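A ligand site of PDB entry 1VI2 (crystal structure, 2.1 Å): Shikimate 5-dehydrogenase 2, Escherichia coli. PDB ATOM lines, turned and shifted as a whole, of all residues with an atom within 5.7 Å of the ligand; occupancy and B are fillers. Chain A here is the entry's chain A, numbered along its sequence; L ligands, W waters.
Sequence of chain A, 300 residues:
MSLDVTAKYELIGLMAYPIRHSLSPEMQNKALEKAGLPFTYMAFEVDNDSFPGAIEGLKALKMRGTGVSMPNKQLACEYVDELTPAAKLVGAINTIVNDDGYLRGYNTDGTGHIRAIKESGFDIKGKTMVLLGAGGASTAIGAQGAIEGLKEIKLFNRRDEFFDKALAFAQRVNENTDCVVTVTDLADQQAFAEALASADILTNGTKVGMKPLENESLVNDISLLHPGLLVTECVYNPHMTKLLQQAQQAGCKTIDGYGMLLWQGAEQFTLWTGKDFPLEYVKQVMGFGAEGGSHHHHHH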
ATOM      1  N   ASP A 109      -4.358 -21.825 -22.678  1.00  0.00           N
ATOM      2  CA  ASP A 109      -3.346 -20.949 -23.240  1.00  0.00           C
ATOM      3  C   ASP A 109      -2.075 -21.750 -23.513  1.00  0.00           C
ATOM      4  O   ASP A 109      -1.475 -21.592 -24.572  1.00  0.00           O
ATOM      5  CB  ASP A 109      -3.031 -19.807 -22.290  1.00  0.00           C
ATOM      6  CG  ASP A 109      -3.955 -18.630 -22.541  1.00  0.00           C
ATOM      7  OD1 ASP A 109      -3.989 -17.709 -21.714  1.00  0.00           O
ATOM      8  OD2 ASP A 109      -4.638 -18.637 -23.592  1.00  0.00           O
ATOM      9  N   GLY A 133       9.707 -13.949 -20.785  1.00  0.00           N
ATOM     10  CA  GLY A 133       8.622 -13.641 -19.855  1.00  0.00           C
ATOM     11  C   GLY A 133       8.336 -14.764 -18.889  1.00  0.00           C
ATOM     12  O   GLY A 133       8.769 -15.909 -19.040  1.00  0.00           O
ATOM     13  N   ALA A 134       7.565 -14.438 -17.844  1.00  0.00           N
ATOM     14  CA  ALA A 134       7.183 -15.424 -16.859  1.00  0.00           C
ATOM     15  C   ALA A 134       5.797 -15.086 -16.300  1.00  0.00           C
ATOM     16  O   ALA A 134       5.451 -15.578 -15.234  1.00  0.00           O
ATOM     17  CB  ALA A 134       8.214 -15.562 -15.758  1.00  0.00           C
ATOM     18  N   GLY A 135       5.038 -14.315 -17.056  1.00  0.00           N
ATOM     19  CA  GLY A 135       3.674 -13.973 -16.671  1.00  0.00           C
ATOM     20  C   GLY A 135       2.719 -15.120 -16.967  1.00  0.00           C
ATOM     21  O   GLY A 135       3.120 -16.284 -17.073  1.00  0.00           O
ATOM     22  N   GLY A 136       1.452 -14.799 -17.184  1.00  0.00           N
ATOM     23  CA  GLY A 136       0.415 -15.772 -17.443  1.00  0.00           C
ATOM     24  C   GLY A 136       0.651 -16.539 -18.740  1.00  0.00           C
ATOM     25  O   GLY A 136       0.603 -17.771 -18.743  1.00  0.00           O
ATOM     26  N   ALA A 137       0.886 -15.860 -19.854  1.00  0.00           N
ATOM     27  CA  ALA A 137       1.128 -16.541 -21.128  1.00  0.00           C
ATOM     28  C   ALA A 137       2.362 -17.398 -21.110  1.00  0.00           C
ATOM     29  O   ALA A 137       2.250 -18.644 -21.348  1.00  0.00           O
ATOM     30  CB  ALA A 137       1.169 -15.521 -22.259  1.00  0.00           C
ATOM     31  N   SER A 138       3.516 -16.875 -20.677  1.00  0.00           N
ATOM     32  CA  SER A 138       4.735 -17.642 -20.641  1.00  0.00           C
ATOM     33  C   SER A 138       4.750 -18.852 -19.747  1.00  0.00           C
ATOM     34  O   SER A 138       5.196 -19.949 -20.153  1.00  0.00           O
ATOM     35  CB  SER A 138       5.959 -16.761 -20.323  1.00  0.00           C
ATOM     36  OG  SER A 138       6.054 -15.673 -21.223  1.00  0.00           O
ATOM     37  N   ASN A 157      13.731 -13.437 -18.352  1.00  0.00           N
ATOM     38  CA  ASN A 157      12.843 -12.415 -17.814  1.00  0.00           C
ATOM     39  C   ASN A 157      13.665 -11.304 -17.158  1.00  0.00           C
ATOM     40  O   ASN A 157      14.646 -11.603 -16.444  1.00  0.00           O
ATOM     41  CB  ASN A 157      11.896 -13.053 -16.804  1.00  0.00           C
ATOM     42  CG  ASN A 157      10.693 -12.214 -16.461  1.00  0.00           C
ATOM     43  OD1 ASN A 157       9.606 -12.382 -17.031  1.00  0.00           O
ATOM     44  ND2 ASN A 157      10.880 -11.287 -15.523  1.00  0.00           N
ATOM     45  N   ARG A 158      13.327 -10.037 -17.409  1.00  0.00           N
ATOM     46  CA  ARG A 158      14.061  -8.957 -16.731  1.00  0.00           C
ATOM     47  C   ARG A 158      13.914  -9.053 -15.224  1.00  0.00           C
ATOM     48  O   ARG A 158      13.155  -9.870 -14.681  1.00  0.00           O
ATOM     49  CB  ARG A 158      13.588  -7.584 -17.219  1.00  0.00           C
ATOM     50  CG  ARG A 158      12.225  -7.161 -16.789  1.00  0.00           C
ATOM     51  CD  ARG A 158      11.752  -5.896 -17.489  1.00  0.00           C
ATOM     52  NE  ARG A 158      10.319  -5.651 -17.265  1.00  0.00           N
ATOM     53  CZ  ARG A 158       9.671  -4.572 -17.692  1.00  0.00           C
ATOM     54  NH1 ARG A 158      10.311  -3.609 -18.358  1.00  0.00           N
ATOM     55  NH2 ARG A 158       8.375  -4.446 -17.490  1.00  0.00           N
ATOM     56  N   ASP A 160      12.097  -7.732 -12.846  1.00  0.00           N
ATOM     57  CA  ASP A 160      10.922  -6.958 -12.421  1.00  0.00           C
ATOM     58  C   ASP A 160      10.141  -7.757 -11.400  1.00  0.00           C
ATOM     59  O   ASP A 160      10.670  -8.721 -10.828  1.00  0.00           O
ATOM     60  CB  ASP A 160      10.057  -6.548 -13.577  1.00  0.00           C
ATOM     61  CG  ASP A 160       9.581  -7.705 -14.464  1.00  0.00           C
ATOM     62  OD1 ASP A 160       9.742  -8.879 -14.050  1.00  0.00           O
ATOM     63  OD2 ASP A 160       9.065  -7.357 -15.567  1.00  0.00           O
ATOM     64  N   PHE A 162       8.140 -10.102 -11.889  1.00  0.00           N
ATOM     65  CA  PHE A 162       7.982 -11.481 -12.315  1.00  0.00           C
ATOM     66  C   PHE A 162       9.217 -12.343 -12.161  1.00  0.00           C
ATOM     67  O   PHE A 162       9.140 -13.590 -12.290  1.00  0.00           O
ATOM     68  CB  PHE A 162       7.514 -11.529 -13.768  1.00  0.00           C
ATOM     69  CG  PHE A 162       6.173 -10.853 -13.972  1.00  0.00           C
ATOM     70  CD1 PHE A 162       6.134  -9.502 -14.309  1.00  0.00           C
ATOM     71  CD2 PHE A 162       5.001 -11.536 -13.809  1.00  0.00           C
ATOM     72  CE1 PHE A 162       4.926  -8.858 -14.468  1.00  0.00           C
ATOM     73  CE2 PHE A 162       3.766 -10.893 -13.994  1.00  0.00           C
ATOM     74  CZ  PHE A 162       3.751  -9.558 -14.319  1.00  0.00           C
ATOM     75  N   LEU A 186      17.436 -11.003 -18.403  1.00  0.00           N
ATOM     76  CA  LEU A 186      17.474 -10.455 -19.744  1.00  0.00           C
ATOM     77  C   LEU A 186      18.662  -9.536 -19.940  1.00  0.00           C
ATOM     78  O   LEU A 186      19.179  -9.431 -21.048  1.00  0.00           O
ATOM     79  CB  LEU A 186      16.185  -9.685 -20.040  1.00  0.00           C
ATOM     80  CG  LEU A 186      15.816  -9.527 -21.519  1.00  0.00           C
ATOM     81  CD1 LEU A 186      14.296  -9.382 -21.667  1.00  0.00           C
ATOM     82  CD2 LEU A 186      16.527  -8.307 -22.116  1.00  0.00           C
ATOM     83  N   ASN A 204       7.759 -15.365 -27.664  1.00  0.00           N
ATOM     84  CA  ASN A 204       7.556 -14.128 -26.921  1.00  0.00           C
ATOM     85  C   ASN A 204       6.216 -14.229 -26.137  1.00  0.00           C
ATOM     86  O   ASN A 204       5.154 -14.329 -26.735  1.00  0.00           O
ATOM     87  CB  ASN A 204       7.447 -12.917 -27.868  1.00  0.00           C
ATOM     88  CG  ASN A 204       7.105 -11.655 -27.065  1.00  0.00           C
ATOM     89  OD1 ASN A 204       7.742 -11.428 -26.047  1.00  0.00           O
ATOM     90  ND2 ASN A 204       6.104 -10.892 -27.492  1.00  0.00           N
ATOM     91  N   GLY A 205       6.333 -14.303 -24.821  1.00  0.00           N
ATOM     92  CA  GLY A 205       5.118 -14.269 -23.994  1.00  0.00           C
ATOM     93  C   GLY A 205       5.030 -12.960 -23.203  1.00  0.00           C
ATOM     94  O   GLY A 205       4.343 -12.949 -22.171  1.00  0.00           O
ATOM     95  N   THR A 206       5.851 -11.967 -23.571  1.00  0.00           N
ATOM     96  CA  THR A 206       5.835 -10.681 -22.867  1.00  0.00           C
ATOM     97  C   THR A 206       4.904  -9.711 -23.580  1.00  0.00           C
ATOM     98  O   THR A 206       4.458 -10.006 -24.704  1.00  0.00           O
ATOM     99  CB  THR A 206       7.206  -9.997 -22.745  1.00  0.00           C
ATOM    100  OG1 THR A 206       7.669  -9.574 -24.016  1.00  0.00           O
ATOM    101  CG2 THR A 206       8.236 -10.864 -22.056  1.00  0.00           C
ATOM    102  N   LYS A 207       4.668  -8.557 -22.981  1.00  0.00           N
ATOM    103  CA  LYS A 207       3.822  -7.538 -23.593  1.00  0.00           C
ATOM    104  C   LYS A 207       4.519  -6.737 -24.670  1.00  0.00           C
ATOM    105  O   LYS A 207       3.912  -5.924 -25.395  1.00  0.00           O
ATOM    106  CB  LYS A 207       3.306  -6.558 -22.502  1.00  0.00           C
ATOM    107  CG  LYS A 207       2.579  -7.305 -21.382  1.00  0.00           C
ATOM    108  CD  LYS A 207       2.234  -6.337 -20.258  1.00  0.00           C
ATOM    109  CE  LYS A 207       0.747  -6.002 -20.273  1.00  0.00           C
ATOM    110  NZ  LYS A 207      -0.034  -7.014 -19.504  1.00  0.00           N
ATOM    111  N   VAL A 208       5.836  -6.860 -24.737  1.00  0.00           N
ATOM    112  CA  VAL A 208       6.608  -6.186 -25.793  1.00  0.00           C
ATOM    113  C   VAL A 208       6.080  -6.592 -27.175  1.00  0.00           C
ATOM    114  O   VAL A 208       5.973  -7.779 -27.482  1.00  0.00           O
ATOM    115  CB  VAL A 208       8.094  -6.523 -25.693  1.00  0.00           C
ATOM    116  CG1 VAL A 208       8.884  -5.773 -26.763  1.00  0.00           C
ATOM    117  CG2 VAL A 208       8.670  -6.200 -24.324  1.00  0.00           C
ATOM    118  N   MET A 210       3.050  -5.554 -28.321  1.00  0.00           N
ATOM    119  CA  MET A 210       1.664  -5.156 -28.213  1.00  0.00           C
ATOM    120  C   MET A 210       1.587  -3.636 -28.013  1.00  0.00           C
ATOM    121  O   MET A 210       2.344  -3.091 -27.207  1.00  0.00           O
ATOM    122  CB  MET A 210       0.980  -5.839 -26.998  1.00  0.00           C
ATOM    123  CG  MET A 210      -0.527  -5.622 -26.915  1.00  0.00           C
ATOM    124  SD  MET A 210      -1.337  -6.392 -25.346  1.00  0.00           S
ATOM    125  CE  MET A 210      -0.283  -5.765 -23.966  1.00  0.00           C
ATOM    126  N   LEU A 213       3.487  -0.289 -26.903  1.00  0.00           N
ATOM    127  CA  LEU A 213       4.829  -0.770 -27.110  1.00  0.00           C
ATOM    128  C   LEU A 213       4.987  -1.536 -28.431  1.00  0.00           C
ATOM    129  O   LEU A 213       5.973  -2.291 -28.563  1.00  0.00           O
ATOM    130  CB  LEU A 213       5.216  -1.757 -25.991  1.00  0.00           C
ATOM    131  CG  LEU A 213       5.815  -1.246 -24.712  1.00  0.00           C
ATOM    132  CD1 LEU A 213       6.147  -2.406 -23.779  1.00  0.00           C
ATOM    133  CD2 LEU A 213       7.072  -0.421 -24.961  1.00  0.00           C
ATOM    134  N   GLU A 216       8.741  -2.382 -30.801  1.00  0.00           N
ATOM    135  CA  GLU A 216       9.931  -2.950 -30.190  1.00  0.00           C
ATOM    136  C   GLU A 216       9.839  -4.458 -29.965  1.00  0.00           C
ATOM    137  O   GLU A 216       8.773  -5.034 -29.880  1.00  0.00           O
ATOM    138  CB  GLU A 216      10.289  -2.237 -28.894  1.00  0.00           C
ATOM    139  CG  GLU A 216       9.464  -2.606 -27.685  1.00  0.00           C
ATOM    140  CD  GLU A 216       9.969  -1.928 -26.422  1.00  0.00           C
ATOM    141  OE1 GLU A 216      10.075  -0.675 -26.436  1.00  0.00           O
ATOM    142  OE2 GLU A 216      10.266  -2.630 -25.445  1.00  0.00           O
ATOM    143  N   LEU A 218      12.247  -7.847 -27.907  1.00  0.00           N
ATOM    144  CA  LEU A 218      13.331  -8.172 -27.010  1.00  0.00           C
ATOM    145  C   LEU A 218      14.564  -8.704 -27.730  1.00  0.00           C
ATOM    146  O   LEU A 218      15.476  -9.241 -27.079  1.00  0.00           O
ATOM    147  CB  LEU A 218      12.852  -9.170 -25.955  1.00  0.00           C
ATOM    148  CG  LEU A 218      11.852  -8.548 -24.942  1.00  0.00           C
ATOM    149  CD1 LEU A 218      11.217  -9.639 -24.112  1.00  0.00           C
ATOM    150  CD2 LEU A 218      12.590  -7.544 -24.064  1.00  0.00           C
ATOM    151  N   GLU A 233       4.718 -15.936 -31.530  1.00  0.00           N
ATOM    152  CA  GLU A 233       4.342 -14.662 -30.875  1.00  0.00           C
ATOM    153  C   GLU A 233       3.004 -14.783 -30.171  1.00  0.00           C
ATOM    154  O   GLU A 233       2.036 -15.284 -30.736  1.00  0.00           O
ATOM    155  CB  GLU A 233       4.228 -13.629 -32.011  1.00  0.00           C
ATOM    156  CG  GLU A 233       3.697 -12.257 -31.634  1.00  0.00           C
ATOM    157  CD  GLU A 233       4.617 -11.530 -30.663  1.00  0.00           C
ATOM    158  OE1 GLU A 233       4.504 -11.789 -29.445  1.00  0.00           O
ATOM    159  OE2 GLU A 233       5.521 -10.834 -31.146  1.00  0.00           O
ATOM    160  N   CYS A 234       2.915 -14.300 -28.936  1.00  0.00           N
ATOM    161  CA  CYS A 234       1.621 -14.291 -28.226  1.00  0.00           C
ATOM    162  C   CYS A 234       0.794 -13.069 -28.592  1.00  0.00           C
ATOM    163  O   CYS A 234      -0.431 -13.078 -28.563  1.00  0.00           O
ATOM    164  CB  CYS A 234       1.854 -14.334 -26.715  1.00  0.00           C
ATOM    165  SG  CYS A 234       2.292 -15.948 -26.054  1.00  0.00           S
ATOM    166  N   VAL A 235       1.474 -11.975 -28.910  1.00  0.00           N
ATOM    167  CA  VAL A 235       0.785 -10.719 -29.212  1.00  0.00           C
ATOM    168  C   VAL A 235      -0.031 -10.866 -30.476  1.00  0.00           C
ATOM    169  O   VAL A 235       0.462 -11.444 -31.468  1.00  0.00           O
ATOM    170  CB  VAL A 235       1.793  -9.551 -29.359  1.00  0.00           C
ATOM    171  CG1 VAL A 235       1.136  -8.337 -30.011  1.00  0.00           C
ATOM    172  CG2 VAL A 235       2.383  -9.201 -28.018  1.00  0.00           C
ATOM    173  N   TYR A 236      -1.288 -10.449 -30.434  1.00  0.00           N
ATOM    174  CA  TYR A 236      -2.136 -10.541 -31.621  1.00  0.00           C
ATOM    175  C   TYR A 236      -2.649  -9.160 -32.013  1.00  0.00           C
ATOM    176  O   TYR A 236      -3.267  -9.017 -33.057  1.00  0.00           O
ATOM    177  CB  TYR A 236      -3.264 -11.526 -31.469  1.00  0.00           C
ATOM    178  CG  TYR A 236      -4.304 -11.187 -30.434  1.00  0.00           C
ATOM    179  CD1 TYR A 236      -5.301 -10.257 -30.675  1.00  0.00           C
ATOM    180  CD2 TYR A 236      -4.305 -11.835 -29.193  1.00  0.00           C
ATOM    181  CE1 TYR A 236      -6.250  -9.942 -29.731  1.00  0.00           C
ATOM    182  CE2 TYR A 236      -5.273 -11.552 -28.243  1.00  0.00           C
ATOM    183  CZ  TYR A 236      -6.248 -10.614 -28.520  1.00  0.00           C
ATOM    184  OH  TYR A 236      -7.195 -10.311 -27.569  1.00  0.00           O
ATOM    185  N   GLY A 257      -0.090 -14.487 -33.157  1.00  0.00           N
ATOM    186  CA  GLY A 257      -0.968 -14.426 -32.025  1.00  0.00           C
ATOM    187  C   GLY A 257      -2.327 -15.066 -32.275  1.00  0.00           C
ATOM    188  O   GLY A 257      -2.915 -15.621 -31.365  1.00  0.00           O
ATOM    189  N   TYR A 258      -2.825 -14.943 -33.511  1.00  0.00           N
ATOM    190  CA  TYR A 258      -4.075 -15.549 -33.915  1.00  0.00           C
ATOM    191  C   TYR A 258      -4.009 -17.065 -33.898  1.00  0.00           C
ATOM    192  O   TYR A 258      -4.995 -17.746 -33.637  1.00  0.00           O
ATOM    193  CB  TYR A 258      -4.556 -15.049 -35.281  1.00  0.00           C
ATOM    194  CG  TYR A 258      -5.022 -13.600 -35.205  1.00  0.00           C
ATOM    195  CD1 TYR A 258      -5.866 -13.151 -34.214  1.00  0.00           C
ATOM    196  CD2 TYR A 258      -4.595 -12.686 -36.167  1.00  0.00           C
ATOM    197  CE1 TYR A 258      -6.280 -11.821 -34.174  1.00  0.00           C
ATOM    198  CE2 TYR A 258      -4.990 -11.367 -36.134  1.00  0.00           C
ATOM    199  CZ  TYR A 258      -5.831 -10.932 -35.127  1.00  0.00           C
ATOM    200  OH  TYR A 258      -6.240  -9.630 -35.064  1.00  0.00           O
ATOM    201  N   MET A 260      -2.295 -18.947 -31.686  1.00  0.00           N
ATOM    202  CA  MET A 260      -2.565 -19.324 -30.296  1.00  0.00           C
ATOM    203  C   MET A 260      -4.012 -19.049 -29.911  1.00  0.00           C
ATOM    204  O   MET A 260      -4.677 -19.948 -29.360  1.00  0.00           O
ATOM    205  CB  MET A 260      -1.660 -18.493 -29.398  1.00  0.00           C
ATOM    206  CG  MET A 260      -1.687 -18.879 -27.928  1.00  0.00           C
ATOM    207  SD  MET A 260      -0.754 -17.557 -26.895  1.00  0.00           S
ATOM    208  CE  MET A 260      -0.969 -18.347 -25.146  1.00  0.00           C
ATOM    209  N   LEU A 261      -4.513 -17.852 -30.241  1.00  0.00           N
ATOM    210  CA  LEU A 261      -5.895 -17.489 -29.888  1.00  0.00           C
ATOM    211  C   LEU A 261      -6.920 -18.498 -30.405  1.00  0.00           C
ATOM    212  O   LEU A 261      -7.879 -18.847 -29.693  1.00  0.00           O
ATOM    213  CB  LEU A 261      -6.258 -16.110 -30.431  1.00  0.00           C
ATOM    214  CG  LEU A 261      -7.629 -15.527 -30.092  1.00  0.00           C
ATOM    215  CD1 LEU A 261      -7.838 -15.449 -28.595  1.00  0.00           C
ATOM    216  CD2 LEU A 261      -7.744 -14.133 -30.718  1.00  0.00           C
ATOM    217  N   GLN A 264      -6.418 -22.052 -28.816  1.00  0.00           N
ATOM    218  CA  GLN A 264      -6.799 -21.971 -27.397  1.00  0.00           C
ATOM    219  C   GLN A 264      -8.322 -22.063 -27.324  1.00  0.00           C
ATOM    220  O   GLN A 264      -8.870 -22.724 -26.454  1.00  0.00           O
ATOM    221  CB  GLN A 264      -6.342 -20.633 -26.827  1.00  0.00           C
ATOM    222  CG  GLN A 264      -6.833 -20.260 -25.459  1.00  0.00           C
ATOM    223  CD  GLN A 264      -8.288 -19.848 -25.384  1.00  0.00           C
ATOM    224  OE1 GLN A 264      -9.018 -20.432 -24.599  1.00  0.00           O
ATOM    225  NE2 GLN A 264      -8.759 -18.967 -26.281  1.00  0.00           N
HETATM  226  P1  LIG L   1       1.497 -10.709 -17.720  1.00  0.00           P
HETATM  227  O1  LIG L   1       1.094  -9.327 -17.188  1.00  0.00           O
HETATM  228  O2  LIG L   1       1.038 -11.755 -16.799  1.00  0.00           O
HETATM  229  O3  LIG L   1       3.095 -10.743 -17.772  1.00  0.00           O
HETATM  230  C1  LIG L   1       3.805  -9.938 -18.796  1.00  0.00           C
HETATM  231  C2  LIG L   1       5.244 -10.435 -18.935  1.00  0.00           C
HETATM  232  O4  LIG L   1       5.890  -9.480 -19.839  1.00  0.00           O
HETATM  233  C3  LIG L   1       6.084 -10.473 -17.687  1.00  0.00           C
HETATM  234  O5  LIG L   1       6.915 -11.638 -17.529  1.00  0.00           O
HETATM  235  C4  LIG L   1       7.019  -9.246 -17.800  1.00  0.00           C
HETATM  236  O6  LIG L   1       8.177  -9.448 -17.034  1.00  0.00           O
HETATM  237  C5  LIG L   1       7.178  -9.121 -19.302  1.00  0.00           C
HETATM  238  N1  LIG L   1       7.415  -7.752 -19.781  1.00  0.00           N
HETATM  239  C6  LIG L   1       6.515  -6.744 -19.915  1.00  0.00           C
HETATM  240  N2  LIG L   1       7.069  -5.631 -20.380  1.00  0.00           N
HETATM  241  C7  LIG L   1       8.396  -5.951 -20.527  1.00  0.00           C
HETATM  242  C8  LIG L   1       9.481  -5.172 -20.985  1.00  0.00           C
HETATM  243  N3  LIG L   1       9.312  -3.907 -21.349  1.00  0.00           N
HETATM  244  N4  LIG L   1      10.694  -5.791 -21.032  1.00  0.00           N
HETATM  245  C9  LIG L   1      10.778  -7.111 -20.633  1.00  0.00           C
HETATM  246  N5  LIG L   1       9.835  -7.910 -20.181  1.00  0.00           N
HETATM  247  C10 LIG L   1       8.636  -7.251 -20.168  1.00  0.00           C
HETATM  248  O7  LIG L   1       1.010 -10.820 -19.207  1.00  0.00           O
HETATM  249  P2  LIG L   1       0.290 -12.005 -20.036  1.00  0.00           P
HETATM  250  O8  LIG L   1      -1.110 -12.215 -19.599  1.00  0.00           O
HETATM  251  O9  LIG L   1       1.100 -13.223 -19.792  1.00  0.00           O
HETATM  252  O10 LIG L   1       0.250 -11.388 -21.499  1.00  0.00           O
HETATM  253  C11 LIG L   1       1.441 -11.354 -22.302  1.00  0.00           C
HETATM  254  C12 LIG L   1       1.116 -10.971 -23.737  1.00  0.00           C
HETATM  255  O11 LIG L   1       0.486 -12.147 -24.359  1.00  0.00           O
HETATM  256  C13 LIG L   1       0.173  -9.817 -23.937  1.00  0.00           C
HETATM  257  O12 LIG L   1       0.476  -9.125 -25.158  1.00  0.00           O
HETATM  258  C14 LIG L   1      -1.213 -10.545 -24.121  1.00  0.00           C
HETATM  259  O13 LIG L   1      -1.977  -9.731 -25.034  1.00  0.00           O
HETATM  260  C15 LIG L   1      -0.766 -11.799 -24.871  1.00  0.00           C
HETATM  261  N6  LIG L   1      -1.673 -12.928 -24.821  1.00  0.00           N
HETATM  262  C16 LIG L   1      -2.088 -13.446 -26.016  1.00  0.00           C
HETATM  263  C17 LIG L   1      -2.915 -14.534 -26.025  1.00  0.00           C
HETATM  264  C18 LIG L   1      -3.388 -15.246 -27.327  1.00  0.00           C
HETATM  265  O14 LIG L   1      -4.190 -16.146 -27.235  1.00  0.00           O
HETATM  266  N7  LIG L   1      -2.729 -14.908 -28.454  1.00  0.00           N
HETATM  267  C19 LIG L   1      -3.370 -15.206 -24.838  1.00  0.00           C
HETATM  268  C20 LIG L   1      -2.848 -14.604 -23.675  1.00  0.00           C
HETATM  269  C21 LIG L   1      -2.080 -13.477 -23.566  1.00  0.00           C
HETATM  270  O   HOH W   1       3.794 -13.961 -19.815  1.00  0.00           O
HETATM  271  O   HOH W   2      10.669 -10.390 -18.774  1.00  0.00           O
HETATM  272  O   HOH W   3      -4.346  -8.072 -25.395  1.00  0.00           O
HETATM  273  O   HOH W   4      13.338  -4.763 -21.461  1.00  0.00           O
HETATM  274  O   HOH W   5      -2.630 -14.343 -19.794  1.00  0.00           O
HETATM  275  O   HOH W   6      11.598  -3.184 -23.009  1.00  0.00           O
HETATM  276  O   HOH W   7      -2.075  -8.912 -27.875  1.00  0.00           O
HETATM  277  O   HOH W   8       0.777 -12.857 -14.385  1.00  0.00           O
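An oxygen (O9) of the ligand lies within hydrogen-bond range of the backbone NH of Ala 137, at 2.6 Å.
The side-chain carboxylate (OD2) of Asp 160 lies within hydrogen-bond range of an oxygen (O6) of the ligand.
The side-chain amide oxygen (OD1) of Asn 157 is in hydrogen-bond range of an oxygen (O5) of the ligand (2.8 Å).
The backbone NH of Ala 134 is in hydrogen-bond range of an oxygen (O5) of the ligand (2.9 Å).
O of Cys 234 lies within hydrogen-bond range of N7 of the ligand, 2.9 Å away.
A nitrogen (N7) of the ligand sits at hydrogen-bond distance from the backbone carbonyl oxygen (O) of Gly 257 (3.0 Å).
An oxygen (O9) of the ligand sits at hydrogen-bond distance from the backbone NH of Gly 136 (3.1 Å).
The guanidinium group of Arg 158 is in hydrogen-bond range of a nitrogen (N2) of the ligand, 3.4 Å away.
The side-chain sulfur of Met 210 is in hydrogen-bond range of an oxygen (O12) of the ligand (3.3 Å).
The backbone NH of Gly 135 sits at hydrogen-bond distance from an oxygen (O5) of the ligand.
The backbone NH (N) of Leu 261 sits close to an oxygen (O14) of the ligand, 3.5 Å away.
The backbone NH (N) of Lys 207 lies within hydrogen-bond range of an oxygen (O4) of the ligand, at 3.5 Å.
The side-chain amino group of Lys 207 lies within salt-bridge range of an oxygen (O1) of the ligand, 3.5 Å away.
N7 of the ligand sits close to SD of Met 260, 3.7 Å away.
The side-chain carboxylate (OD1) of Asp 160 lies within hydrogen-bond range of the side-chain amide nitrogen (ND2) of Asn 157 (3.0 Å).
The side-chain carboxylate of Asp 160 lies within hydrogen-bond range of the backbone NH of Phe 162 (3.0 Å).
N of Ala 134 lies within hydrogen-bond range of OD1 of Asn 157.
The backbone NH of Leu 186 sits at hydrogen-bond distance from the backbone carbonyl oxygen of Asn 157 (3.5 Å).
N of Cys 234 sits at hydrogen-bond distance from O of Asn 204.
N of Gly 257 sits at hydrogen-bond distance from O of Glu 233.
The side-chain hydroxyl (OG1) of Thr 206 lies within hydrogen-bond range of the side-chain amide oxygen (OD1) of Asn 204.
The backbone NH (N) of Val 235 lies within hydrogen-bond range of the side-chain carboxylate (OE1) of Glu 233, at 3.1 Å.
Residues that only touch the ligand: Asp 109 (3.8 Å), Gly 133 (3.5 Å), Phe 162 (3.4 Å), Gly 205 (3.3 Å), Thr 206 (3.2 Å), Val 208 (3.6 Å), Leu 218 (3.9 Å), Val 235 (3.4 Å) and Tyr 236 (3.5 Å).
Hydrophobic or aromatic side chains within 4 Å of the ligand: Ala 137, Phe 162, Val 208, Met 210, Leu 218, Val 235, Tyr 236, Met 260 and Leu 261.
22 residues have an atom within 4 Å of the ligand: Asp 109, Gly 133, Ala 134, Gly 135, Gly 136, Ala 137, Asn 157, Arg 158, Asp 160, Phe 162, Gly 205, Thr 206, Lys 207, Val 208, Met 210, Leu 218, Cys 234, Val 235, Tyr 236, Gly 257, Met 260 and Leu 261.
Along chain A the residues within 4 Å of the ligand span positions 109 to 261.
The nearest printed residue that does not touch the ligand is Leu 213 (4.3 Å).
Water W8 bridges an oxygen (O2) of the ligand (2.7 Å) and the backbone NH (N) of Gly 136 (3.5 Å).
Water W3 bridges O13 of the ligand (2.9 Å) and SD of Met 210 (3.4 Å).
Water W6 lies within hydrogen-bond range of OE2 of Glu 216 (2.8 Å) and N3 of the ligand (2.9 Å).
Water W7 lies within hydrogen-bond range of an oxygen (O13) of the ligand (3.0 Å), the backbone NH (N) of Tyr 236 (3.1 Å) and the side-chain sulfur (SD) of Met 210 (3.6 Å).
Water W2 lies within hydrogen-bond range of OD1 of Asn 157 (2.9 Å), N5 of the ligand (3.0 Å) and N of Arg 158 (3.0 Å).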
